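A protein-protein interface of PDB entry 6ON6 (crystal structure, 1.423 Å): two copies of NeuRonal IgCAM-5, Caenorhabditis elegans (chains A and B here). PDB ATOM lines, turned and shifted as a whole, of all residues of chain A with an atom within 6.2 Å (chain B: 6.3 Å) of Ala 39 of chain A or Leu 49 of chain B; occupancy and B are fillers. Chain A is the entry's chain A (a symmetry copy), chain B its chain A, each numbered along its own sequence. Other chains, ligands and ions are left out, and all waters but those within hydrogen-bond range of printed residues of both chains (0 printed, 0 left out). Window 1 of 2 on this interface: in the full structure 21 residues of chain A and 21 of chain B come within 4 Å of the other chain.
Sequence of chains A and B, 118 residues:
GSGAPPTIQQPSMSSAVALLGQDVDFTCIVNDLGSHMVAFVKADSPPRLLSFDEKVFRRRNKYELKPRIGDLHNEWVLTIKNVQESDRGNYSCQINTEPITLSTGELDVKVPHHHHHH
The backbone carbonyl oxygen (O) of Pro 47 of chain B lies close to the side-chain amide oxygen (OE1) of Gln 94 of chain A. NE2 of Gln 94 of chain A sits close to N of Leu 49 of chain B (2.9 Å). The backbone NH (N) of Ile 100 of chain A sits close to the guanidinium group (NH1) of Arg 58 of chain B (3.2 Å).
N of Lys 42 of chain B lies within hydrogen-bond range of O of Arg 48 of chain B, at 2.9 Å. O of Leu 50 of chain B lies within hydrogen-bond range of N of Phe 57 of chain B, at 2.9 Å. O of Ala 39 of chain A sits at hydrogen-bond distance from N of Gln 94 of chain A (2.8 Å). O of Val 41 of chain A is in hydrogen-bond range of N of Ser 92 of chain A (2.9 Å).
Met 37 of chain A touches Phe 57 of chain B. CB of Ala 39 of chain A touches CD2 of Leu 49 of chain B (3.8 Å). Leu 49 of chain A touches Ala 39 of chain B. CD2 of Leu 49 of chain A touches CD1 of Phe 52 of chain B (3.6 Å). CD2 of Leu 49 of chain B touches CD1 of Phe 52 of chain A (3.6 Å). CD2 of Phe 52 of chain A touches CD2 of Phe 52 of chain B (3.4 Å). Phe 57 of chain B touches Phe 52 of chain A. Gln 94 of chain A touches Arg 48 of chain B (NE2 to CA, 3.7 Å). Gln 94 of chain A touches Phe 57 of chain B. CD of Arg 48 of chain B touches CD1 of Ile 100 of chain A (3.8 Å).
Of chain B, only Leu 49 comes within 4 Å of Ala 39 of chain A. Printed residues of chain A within 4 Å of Leu 49 of chain B: Ala 39, Phe 52 and Gln 94. Printed residues of chain A within 4 Å of Arg 48 of chain B: Gln 94 and Ile 100. Printed residues of chain B within 4 Å of Ile 100 of chain A: Arg 48 (3.8 Å) and Arg 58 (3.2 Å). Ser 92 of chain A touches none of the printed residues of chain B. Ser 51 of chain A touches none of the printed residues of chain B. The nearest residue of chain B that does not touch Ala 39 of chain A is Phe 57 of chain B (4.1 Å). The nearest residue of chain A that does not touch Leu 49 of chain B is Leu 49 of chain A (4.2 Å).
Printed residues of chain A that touch a printed residue of chain B: Met 37, Ala 39, Val 41, Leu 49, Phe 52, Gln 94 and Ile 100. Printed residues of chain B that touch a printed residue of chain A: Ala 39, Pro 47, Arg 48, Leu 49, Phe 52, Phe 57 and Arg 58. Among the printed residues, 14 pairs touch across the chains. Among the printed residues, no Asp or Glu carboxylate lies within 4 Å of a Lys or Arg side-chain nitrogen of the other chain.
Ala 39 of chain A touches Leu 49 of chain B, and with the chains exchanged Leu 49 of chain A touches Ala 39 of chain B. Leu 49 of chain A touches Phe 52 of chain B, and with the chains exchanged Phe 52 of chain A touches Leu 49 of chain B. Phe 52 of chain A touches its own counterpart, Phe 52 of chain B. Positions printed for both chains: 39, 40, 41, 49, 51 and 52.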
ATOM      1  N   MET A  37     -28.103 -14.169  -2.044  1.00  0.00           N
ATOM      2  CA  MET A  37     -26.673 -14.113  -1.743  1.00  0.00           C
ATOM      3  C   MET A  37     -25.857 -14.165  -3.026  1.00  0.00           C
ATOM      4  O   MET A  37     -26.188 -14.918  -3.947  1.00  0.00           O
ATOM      5  CB  MET A  37     -26.297 -15.322  -0.890  1.00  0.00           C
ATOM      6  CG  MET A  37     -26.921 -15.322   0.471  1.00  0.00           C
ATOM      7  SD  MET A  37     -26.121 -14.127   1.548  1.00  0.00           S
ATOM      8  CE  MET A  37     -27.272 -12.766   1.488  1.00  0.00           C
ATOM      9  N   VAL A  38     -24.734 -13.435  -3.034  1.00  0.00           N
ATOM     10  CA  VAL A  38     -23.791 -13.390  -4.151  1.00  0.00           C
ATOM     11  C   VAL A  38     -22.512 -14.101  -3.727  1.00  0.00           C
ATOM     12  O   VAL A  38     -21.966 -13.819  -2.650  1.00  0.00           O
ATOM     13  CB  VAL A  38     -23.435 -11.943  -4.531  1.00  0.00           C
ATOM     14  CG1 VAL A  38     -22.414 -11.902  -5.642  1.00  0.00           C
ATOM     15  CG2 VAL A  38     -24.671 -11.192  -4.993  1.00  0.00           C
ATOM     16  N   ALA A  39     -22.017 -14.982  -4.585  1.00  0.00           N
ATOM     17  CA  ALA A  39     -20.737 -15.646  -4.333  1.00  0.00           C
ATOM     18  C   ALA A  39     -19.855 -15.491  -5.562  1.00  0.00           C
ATOM     19  O   ALA A  39     -20.340 -15.534  -6.684  1.00  0.00           O
ATOM     20  CB  ALA A  39     -20.937 -17.136  -3.995  1.00  0.00           C
ATOM     21  N   PHE A  40     -18.551 -15.298  -5.363  1.00  0.00           N
ATOM     22  CA  PHE A  40     -17.595 -15.308  -6.468  1.00  0.00           C
ATOM     23  C   PHE A  40     -16.777 -16.586  -6.389  1.00  0.00           C
ATOM     24  O   PHE A  40     -16.339 -16.977  -5.307  1.00  0.00           O
ATOM     25  CB  PHE A  40     -16.613 -14.138  -6.399  1.00  0.00           C
ATOM     26  CG  PHE A  40     -17.201 -12.845  -6.865  1.00  0.00           C
ATOM     27  CD1 PHE A  40     -16.945 -12.352  -8.136  1.00  0.00           C
ATOM     28  CD2 PHE A  40     -17.996 -12.099  -6.023  1.00  0.00           C
ATOM     29  CE1 PHE A  40     -17.509 -11.143  -8.569  1.00  0.00           C
ATOM     30  CE2 PHE A  40     -18.555 -10.895  -6.459  1.00  0.00           C
ATOM     31  CZ  PHE A  40     -18.252 -10.410  -7.708  1.00  0.00           C
ATOM     32  N   VAL A  41     -16.583 -17.241  -7.529  1.00  0.00           N
ATOM     33  CA  VAL A  41     -15.889 -18.524  -7.559  1.00  0.00           C
ATOM     34  C   VAL A  41     -14.904 -18.508  -8.728  1.00  0.00           C
ATOM     35  O   VAL A  41     -15.112 -17.829  -9.730  1.00  0.00           O
ATOM     36  CB  VAL A  41     -16.941 -19.652  -7.676  1.00  0.00           C
ATOM     37  CG1 VAL A  41     -16.318 -20.971  -7.761  1.00  0.00           C
ATOM     38  CG2 VAL A  41     -17.890 -19.660  -6.484  1.00  0.00           C
ATOM     39  N   LEU A  49     -13.891 -21.180  -3.846  1.00  0.00           N
ATOM     40  CA  LEU A  49     -14.713 -20.075  -3.387  1.00  0.00           C
ATOM     41  C   LEU A  49     -13.818 -18.876  -3.081  1.00  0.00           C
ATOM     42  O   LEU A  49     -12.819 -18.987  -2.342  1.00  0.00           O
ATOM     43  CB  LEU A  49     -15.515 -20.487  -2.158  1.00  0.00           C
ATOM     44  CG  LEU A  49     -16.425 -19.403  -1.558  1.00  0.00           C
ATOM     45  CD1 LEU A  49     -17.542 -19.020  -2.530  1.00  0.00           C
ATOM     46  CD2 LEU A  49     -17.024 -19.873  -0.220  1.00  0.00           C
ATOM     47  N   SER A  51     -15.424 -15.479  -2.491  1.00  0.00           N
ATOM     48  CA  SER A  51     -16.142 -14.618  -1.563  1.00  0.00           C
ATOM     49  C   SER A  51     -17.556 -15.130  -1.437  1.00  0.00           C
ATOM     50  O   SER A  51     -18.065 -15.784  -2.346  1.00  0.00           O
ATOM     51  CB  SER A  51     -16.175 -13.154  -2.005  1.00  0.00           C
ATOM     52  OG  SER A  51     -16.906 -13.015  -3.228  1.00  0.00           O
ATOM     53  N   PHE A  52     -18.171 -14.834  -0.296  1.00  0.00           N
ATOM     54  CA  PHE A  52     -19.565 -15.170  -0.037  1.00  0.00           C
ATOM     55  C   PHE A  52     -20.228 -13.966   0.604  1.00  0.00           C
ATOM     56  O   PHE A  52     -19.728 -13.445   1.604  1.00  0.00           O
ATOM     57  CB  PHE A  52     -19.680 -16.377   0.903  1.00  0.00           C
ATOM     58  CG  PHE A  52     -21.098 -16.757   1.174  1.00  0.00           C
ATOM     59  CD1 PHE A  52     -21.840 -17.465   0.242  1.00  0.00           C
ATOM     60  CD2 PHE A  52     -21.721 -16.340   2.329  1.00  0.00           C
ATOM     61  CE1 PHE A  52     -23.164 -17.781   0.474  1.00  0.00           C
ATOM     62  CE2 PHE A  52     -23.057 -16.648   2.559  1.00  0.00           C
ATOM     63  CZ  PHE A  52     -23.775 -17.370   1.632  1.00  0.00           C
ATOM     64  N   ASP A  53     -21.355 -13.527   0.041  1.00  0.00           N
ATOM     65  CA  ASP A  53     -22.014 -12.344   0.582  1.00  0.00           C
ATOM     66  C   ASP A  53     -20.982 -11.214   0.645  1.00  0.00           C
ATOM     67  O   ASP A  53     -20.358 -10.905  -0.377  1.00  0.00           O
ATOM     68  CB  ASP A  53     -22.671 -12.703   1.928  1.00  0.00           C
ATOM     69  CG  ASP A  53     -23.675 -11.664   2.413  1.00  0.00           C
ATOM     70  OD1 ASP A  53     -24.150 -10.835   1.606  1.00  0.00           O
ATOM     71  OD2 ASP A  53     -23.977 -11.682   3.631  1.00  0.00           O
ATOM     72  N   SER A  92     -16.461 -16.437 -11.865  1.00  0.00           N
ATOM     73  CA  SER A  92     -17.896 -16.298 -12.024  1.00  0.00           C
ATOM     74  C   SER A  92     -18.516 -15.665 -10.778  1.00  0.00           C
ATOM     75  O   SER A  92     -18.042 -15.841  -9.655  1.00  0.00           O
ATOM     76  CB  SER A  92     -18.479 -17.655 -12.443  1.00  0.00           C
ATOM     77  OG  SER A  92     -18.497 -18.509 -11.339  1.00  0.00           O
ATOM     78  N   CYS A  93     -19.570 -14.876 -10.962  1.00  0.00           N
ATOM     79  CA  CYS A  93     -20.363 -14.487  -9.810  1.00  0.00           C
ATOM     80  C   CYS A  93     -21.674 -15.231  -9.935  1.00  0.00           C
ATOM     81  O   CYS A  93     -22.188 -15.401 -11.043  1.00  0.00           O
ATOM     82  CB  CYS A  93     -20.584 -12.971  -9.663  1.00  0.00           C
ATOM     83  SG  CYS A  93     -21.741 -12.312 -10.724  1.00  0.00           S
ATOM     84  N   GLN A  94     -22.167 -15.727  -8.824  1.00  0.00           N
ATOM     85  CA  GLN A  94     -23.368 -16.542  -8.847  1.00  0.00           C
ATOM     86  C   GLN A  94     -24.289 -16.139  -7.710  1.00  0.00           C
ATOM     87  O   GLN A  94     -23.823 -15.754  -6.634  1.00  0.00           O
ATOM     88  CB  GLN A  94     -23.007 -18.015  -8.897  1.00  0.00           C
ATOM     89  CG  GLN A  94     -22.377 -18.525  -7.709  1.00  0.00           C
ATOM     90  CD  GLN A  94     -21.831 -19.943  -7.945  1.00  0.00           C
ATOM     91  OE1 GLN A  94     -20.940 -20.155  -8.776  1.00  0.00           O
ATOM     92  NE2 GLN A  94     -22.410 -20.909  -7.273  1.00  0.00           N
ATOM     93  N   ILE A  95     -25.608 -16.115  -8.003  1.00  0.00           N
ATOM     94  CA  ILE A  95     -26.620 -15.731  -7.035  1.00  0.00           C
ATOM     95  C   ILE A  95     -27.497 -16.932  -6.768  1.00  0.00           C
ATOM     96  O   ILE A  95     -27.763 -17.707  -7.689  1.00  0.00           O
ATOM     97  CB  ILE A  95     -27.496 -14.627  -7.641  1.00  0.00           C
ATOM     98  CG1 ILE A  95     -26.613 -13.557  -8.303  1.00  0.00           C
ATOM     99  CG2 ILE A  95     -28.322 -14.018  -6.560  1.00  0.00           C
ATOM    100  CD1 ILE A  95     -27.364 -12.643  -9.267  1.00  0.00           C
ATOM    101  N   ILE A 100     -30.515 -20.756 -10.952  1.00  0.00           N
ATOM    102  CA  ILE A 100     -29.358 -19.935 -10.582  1.00  0.00           C
ATOM    103  C   ILE A 100     -29.203 -18.773 -11.550  1.00  0.00           C
ATOM    104  O   ILE A 100     -29.683 -18.779 -12.678  1.00  0.00           O
ATOM    105  CB  ILE A 100     -28.106 -20.818 -10.571  1.00  0.00           C
ATOM    106  CG1 ILE A 100     -26.963 -20.156  -9.807  1.00  0.00           C
ATOM    107  CG2 ILE A 100     -27.753 -21.161 -12.022  1.00  0.00           C
ATOM    108  CD1 ILE A 100     -25.946 -21.107  -9.424  1.00  0.00           C
ATOM    109  N   ALA B  39     -16.853 -24.795   3.180  1.00  0.00           N
ATOM    110  CA  ALA B  39     -17.728 -24.639   2.018  1.00  0.00           C
ATOM    111  C   ALA B  39     -17.707 -25.928   1.213  1.00  0.00           C
ATOM    112  O   ALA B  39     -16.673 -26.573   1.100  1.00  0.00           O
ATOM    113  CB  ALA B  39     -17.290 -23.447   1.144  1.00  0.00           C
ATOM    114  N   PHE B  40     -18.850 -26.322   0.652  1.00  0.00           N
ATOM    115  CA  PHE B  40     -18.902 -27.448  -0.280  1.00  0.00           C
ATOM    116  C   PHE B  40     -19.133 -26.908  -1.681  1.00  0.00           C
ATOM    117  O   PHE B  40     -19.966 -26.022  -1.874  1.00  0.00           O
ATOM    118  CB  PHE B  40     -20.052 -28.407   0.030  1.00  0.00           C
ATOM    119  CG  PHE B  40     -19.768 -29.318   1.181  1.00  0.00           C
ATOM    120  CD1 PHE B  40     -19.370 -30.632   0.981  1.00  0.00           C
ATOM    121  CD2 PHE B  40     -19.922 -28.873   2.475  1.00  0.00           C
ATOM    122  CE1 PHE B  40     -19.096 -31.478   2.065  1.00  0.00           C
ATOM    123  CE2 PHE B  40     -19.648 -29.720   3.553  1.00  0.00           C
ATOM    124  CZ  PHE B  40     -19.295 -31.027   3.325  1.00  0.00           C
ATOM    125  N   VAL B  41     -18.390 -27.429  -2.650  1.00  0.00           N
ATOM    126  CA  VAL B  41     -18.463 -26.926  -4.018  1.00  0.00           C
ATOM    127  C   VAL B  41     -18.507 -28.122  -4.967  1.00  0.00           C
ATOM    128  O   VAL B  41     -17.986 -29.194  -4.668  1.00  0.00           O
ATOM    129  CB  VAL B  41     -17.247 -26.003  -4.270  1.00  0.00           C
ATOM    130  CG1 VAL B  41     -17.224 -25.495  -5.639  1.00  0.00           C
ATOM    131  CG2 VAL B  41     -17.245 -24.805  -3.329  1.00  0.00           C
ATOM    132  N   LYS B  42     -19.193 -27.969  -6.095  1.00  0.00           N
ATOM    133  CA  LYS B  42     -19.139 -28.954  -7.166  1.00  0.00           C
ATOM    134  C   LYS B  42     -18.259 -28.404  -8.274  1.00  0.00           C
ATOM    135  O   LYS B  42     -18.486 -27.275  -8.741  1.00  0.00           O
ATOM    136  CB  LYS B  42     -20.524 -29.224  -7.761  1.00  0.00           C
ATOM    137  CG  LYS B  42     -20.479 -30.507  -8.564  1.00  0.00           C
ATOM    138  CD  LYS B  42     -21.619 -30.666  -9.474  1.00  0.00           C
ATOM    139  CE  LYS B  42     -21.366 -31.886 -10.309  1.00  0.00           C
ATOM    140  NZ  LYS B  42     -22.385 -31.953 -11.342  1.00  0.00           N
ATOM    141  N   PRO B  47     -18.284 -23.687 -11.740  1.00  0.00           N
ATOM    142  CA  PRO B  47     -18.520 -24.450 -10.515  1.00  0.00           C
ATOM    143  C   PRO B  47     -19.740 -23.906  -9.807  1.00  0.00           C
ATOM    144  O   PRO B  47     -20.276 -22.840 -10.146  1.00  0.00           O
ATOM    145  CB  PRO B  47     -17.260 -24.215  -9.685  1.00  0.00           C
ATOM    146  CG  PRO B  47     -16.633 -23.001 -10.256  1.00  0.00           C
ATOM    147  CD  PRO B  47     -17.051 -22.883 -11.672  1.00  0.00           C
ATOM    148  N   ARG B  48     -20.217 -24.691  -8.853  1.00  0.00           N
ATOM    149  CA  ARG B  48     -21.414 -24.335  -8.112  1.00  0.00           C
ATOM    150  C   ARG B  48     -21.085 -24.391  -6.638  1.00  0.00           C
ATOM    151  O   ARG B  48     -20.671 -25.439  -6.136  1.00  0.00           O
ATOM    152  CB  ARG B  48     -22.511 -25.335  -8.405  1.00  0.00           C
ATOM    153  CG  ARG B  48     -22.990 -25.269  -9.843  1.00  0.00           C
ATOM    154  CD  ARG B  48     -23.509 -23.897 -10.200  1.00  0.00           C
ATOM    155  NE  ARG B  48     -24.137 -23.922 -11.518  1.00  0.00           N
ATOM    156  CZ  ARG B  48     -25.393 -24.314 -11.739  1.00  0.00           C
ATOM    157  NH1 ARG B  48     -26.161 -24.708 -10.725  1.00  0.00           N
ATOM    158  NH2 ARG B  48     -25.882 -24.313 -12.972  1.00  0.00           N
ATOM    159  N   LEU B  49     -21.253 -23.276  -5.948  1.00  0.00           N
ATOM    160  CA  LEU B  49     -21.279 -23.315  -4.496  1.00  0.00           C
ATOM    161  C   LEU B  49     -22.514 -24.087  -4.038  1.00  0.00           C
ATOM    162  O   LEU B  49     -23.651 -23.804  -4.467  1.00  0.00           O
ATOM    163  CB  LEU B  49     -21.275 -21.901  -3.928  1.00  0.00           C
ATOM    164  CG  LEU B  49     -21.313 -21.795  -2.395  1.00  0.00           C
ATOM    165  CD1 LEU B  49     -20.042 -22.372  -1.771  1.00  0.00           C
ATOM    166  CD2 LEU B  49     -21.505 -20.333  -1.954  1.00  0.00           C
ATOM    167  N   LEU B  50     -22.296 -25.085  -3.169  1.00  0.00           N
ATOM    168  CA  LEU B  50     -23.394 -25.884  -2.643  1.00  0.00           C
ATOM    169  C   LEU B  50     -23.763 -25.517  -1.214  1.00  0.00           C
ATOM    170  O   LEU B  50     -24.952 -25.547  -0.874  1.00  0.00           O
ATOM    171  CB  LEU B  50     -23.059 -27.377  -2.713  1.00  0.00           C
ATOM    172  CG  LEU B  50     -22.655 -27.895  -4.082  1.00  0.00           C
ATOM    173  CD1 LEU B  50     -22.295 -29.365  -4.018  1.00  0.00           C
ATOM    174  CD2 LEU B  50     -23.792 -27.695  -5.075  1.00  0.00           C
ATOM    175  N   SER B  51     -22.791 -25.120  -0.387  1.00  0.00           N
ATOM    176  CA  SER B  51     -23.091 -24.703   0.975  1.00  0.00           C
ATOM    177  C   SER B  51     -21.953 -23.845   1.470  1.00  0.00           C
ATOM    178  O   SER B  51     -20.827 -23.966   0.990  1.00  0.00           O
ATOM    179  CB  SER B  51     -23.287 -25.880   1.933  1.00  0.00           C
ATOM    180  OG  SER B  51     -22.072 -26.626   2.067  1.00  0.00           O
ATOM    181  N   PHE B  52     -22.268 -22.973   2.423  1.00  0.00           N
ATOM    182  CA  PHE B  52     -21.280 -22.127   3.080  1.00  0.00           C
ATOM    183  C   PHE B  52     -21.563 -22.142   4.571  1.00  0.00           C
ATOM    184  O   PHE B  52     -22.692 -21.873   4.987  1.00  0.00           O
ATOM    185  CB  PHE B  52     -21.353 -20.685   2.562  1.00  0.00           C
ATOM    186  CG  PHE B  52     -20.341 -19.795   3.205  1.00  0.00           C
ATOM    187  CD1 PHE B  52     -19.011 -19.824   2.814  1.00  0.00           C
ATOM    188  CD2 PHE B  52     -20.698 -18.982   4.257  1.00  0.00           C
ATOM    189  CE1 PHE B  52     -18.066 -19.032   3.436  1.00  0.00           C
ATOM    190  CE2 PHE B  52     -19.745 -18.191   4.891  1.00  0.00           C
ATOM    191  CZ  PHE B  52     -18.433 -18.217   4.478  1.00  0.00           C
ATOM    192  N   PHE B  57     -26.577 -23.258  -0.008  1.00  0.00           N
ATOM    193  CA  PHE B  57     -26.670 -22.037  -0.807  1.00  0.00           C
ATOM    194  C   PHE B  57     -28.067 -21.876  -1.392  1.00  0.00           C
ATOM    195  O   PHE B  57     -28.664 -20.798  -1.320  1.00  0.00           O
ATOM    196  CB  PHE B  57     -25.609 -22.107  -1.911  1.00  0.00           C
ATOM    197  CG  PHE B  57     -25.384 -20.824  -2.662  1.00  0.00           C
ATOM    198  CD1 PHE B  57     -25.157 -19.618  -1.994  1.00  0.00           C
ATOM    199  CD2 PHE B  57     -25.260 -20.853  -4.038  1.00  0.00           C
ATOM    200  CE1 PHE B  57     -24.871 -18.445  -2.700  1.00  0.00           C
ATOM    201  CE2 PHE B  57     -24.984 -19.672  -4.768  1.00  0.00           C
ATOM    202  CZ  PHE B  57     -24.780 -18.472  -4.092  1.00  0.00           C
ATOM    203  N   ARG B  58     -28.608 -22.946  -1.950  1.00  0.00           N
ATOM    204  CA  ARG B  58     -29.893 -22.916  -2.639  1.00  0.00           C
ATOM    205  C   ARG B  58     -30.357 -24.350  -2.785  1.00  0.00           C
ATOM    206  O   ARG B  58     -29.605 -25.284  -2.491  1.00  0.00           O
ATOM    207  CB  ARG B  58     -29.711 -22.302  -4.017  1.00  0.00           C
ATOM    208  CG  ARG B  58     -28.530 -22.910  -4.750  1.00  0.00           C
ATOM    209  CD  ARG B  58     -28.164 -22.143  -6.000  1.00  0.00           C
ATOM    210  NE  ARG B  58     -29.238 -22.183  -6.972  1.00  0.00           N
ATOM    211  CZ  ARG B  58     -29.394 -23.141  -7.881  1.00  0.00           C
ATOM    212  NH1 ARG B  58     -30.418 -23.066  -8.711  1.00  0.00           N
ATOM    213  NH2 ARG B  58     -28.513 -24.138  -7.983  1.00  0.00           N
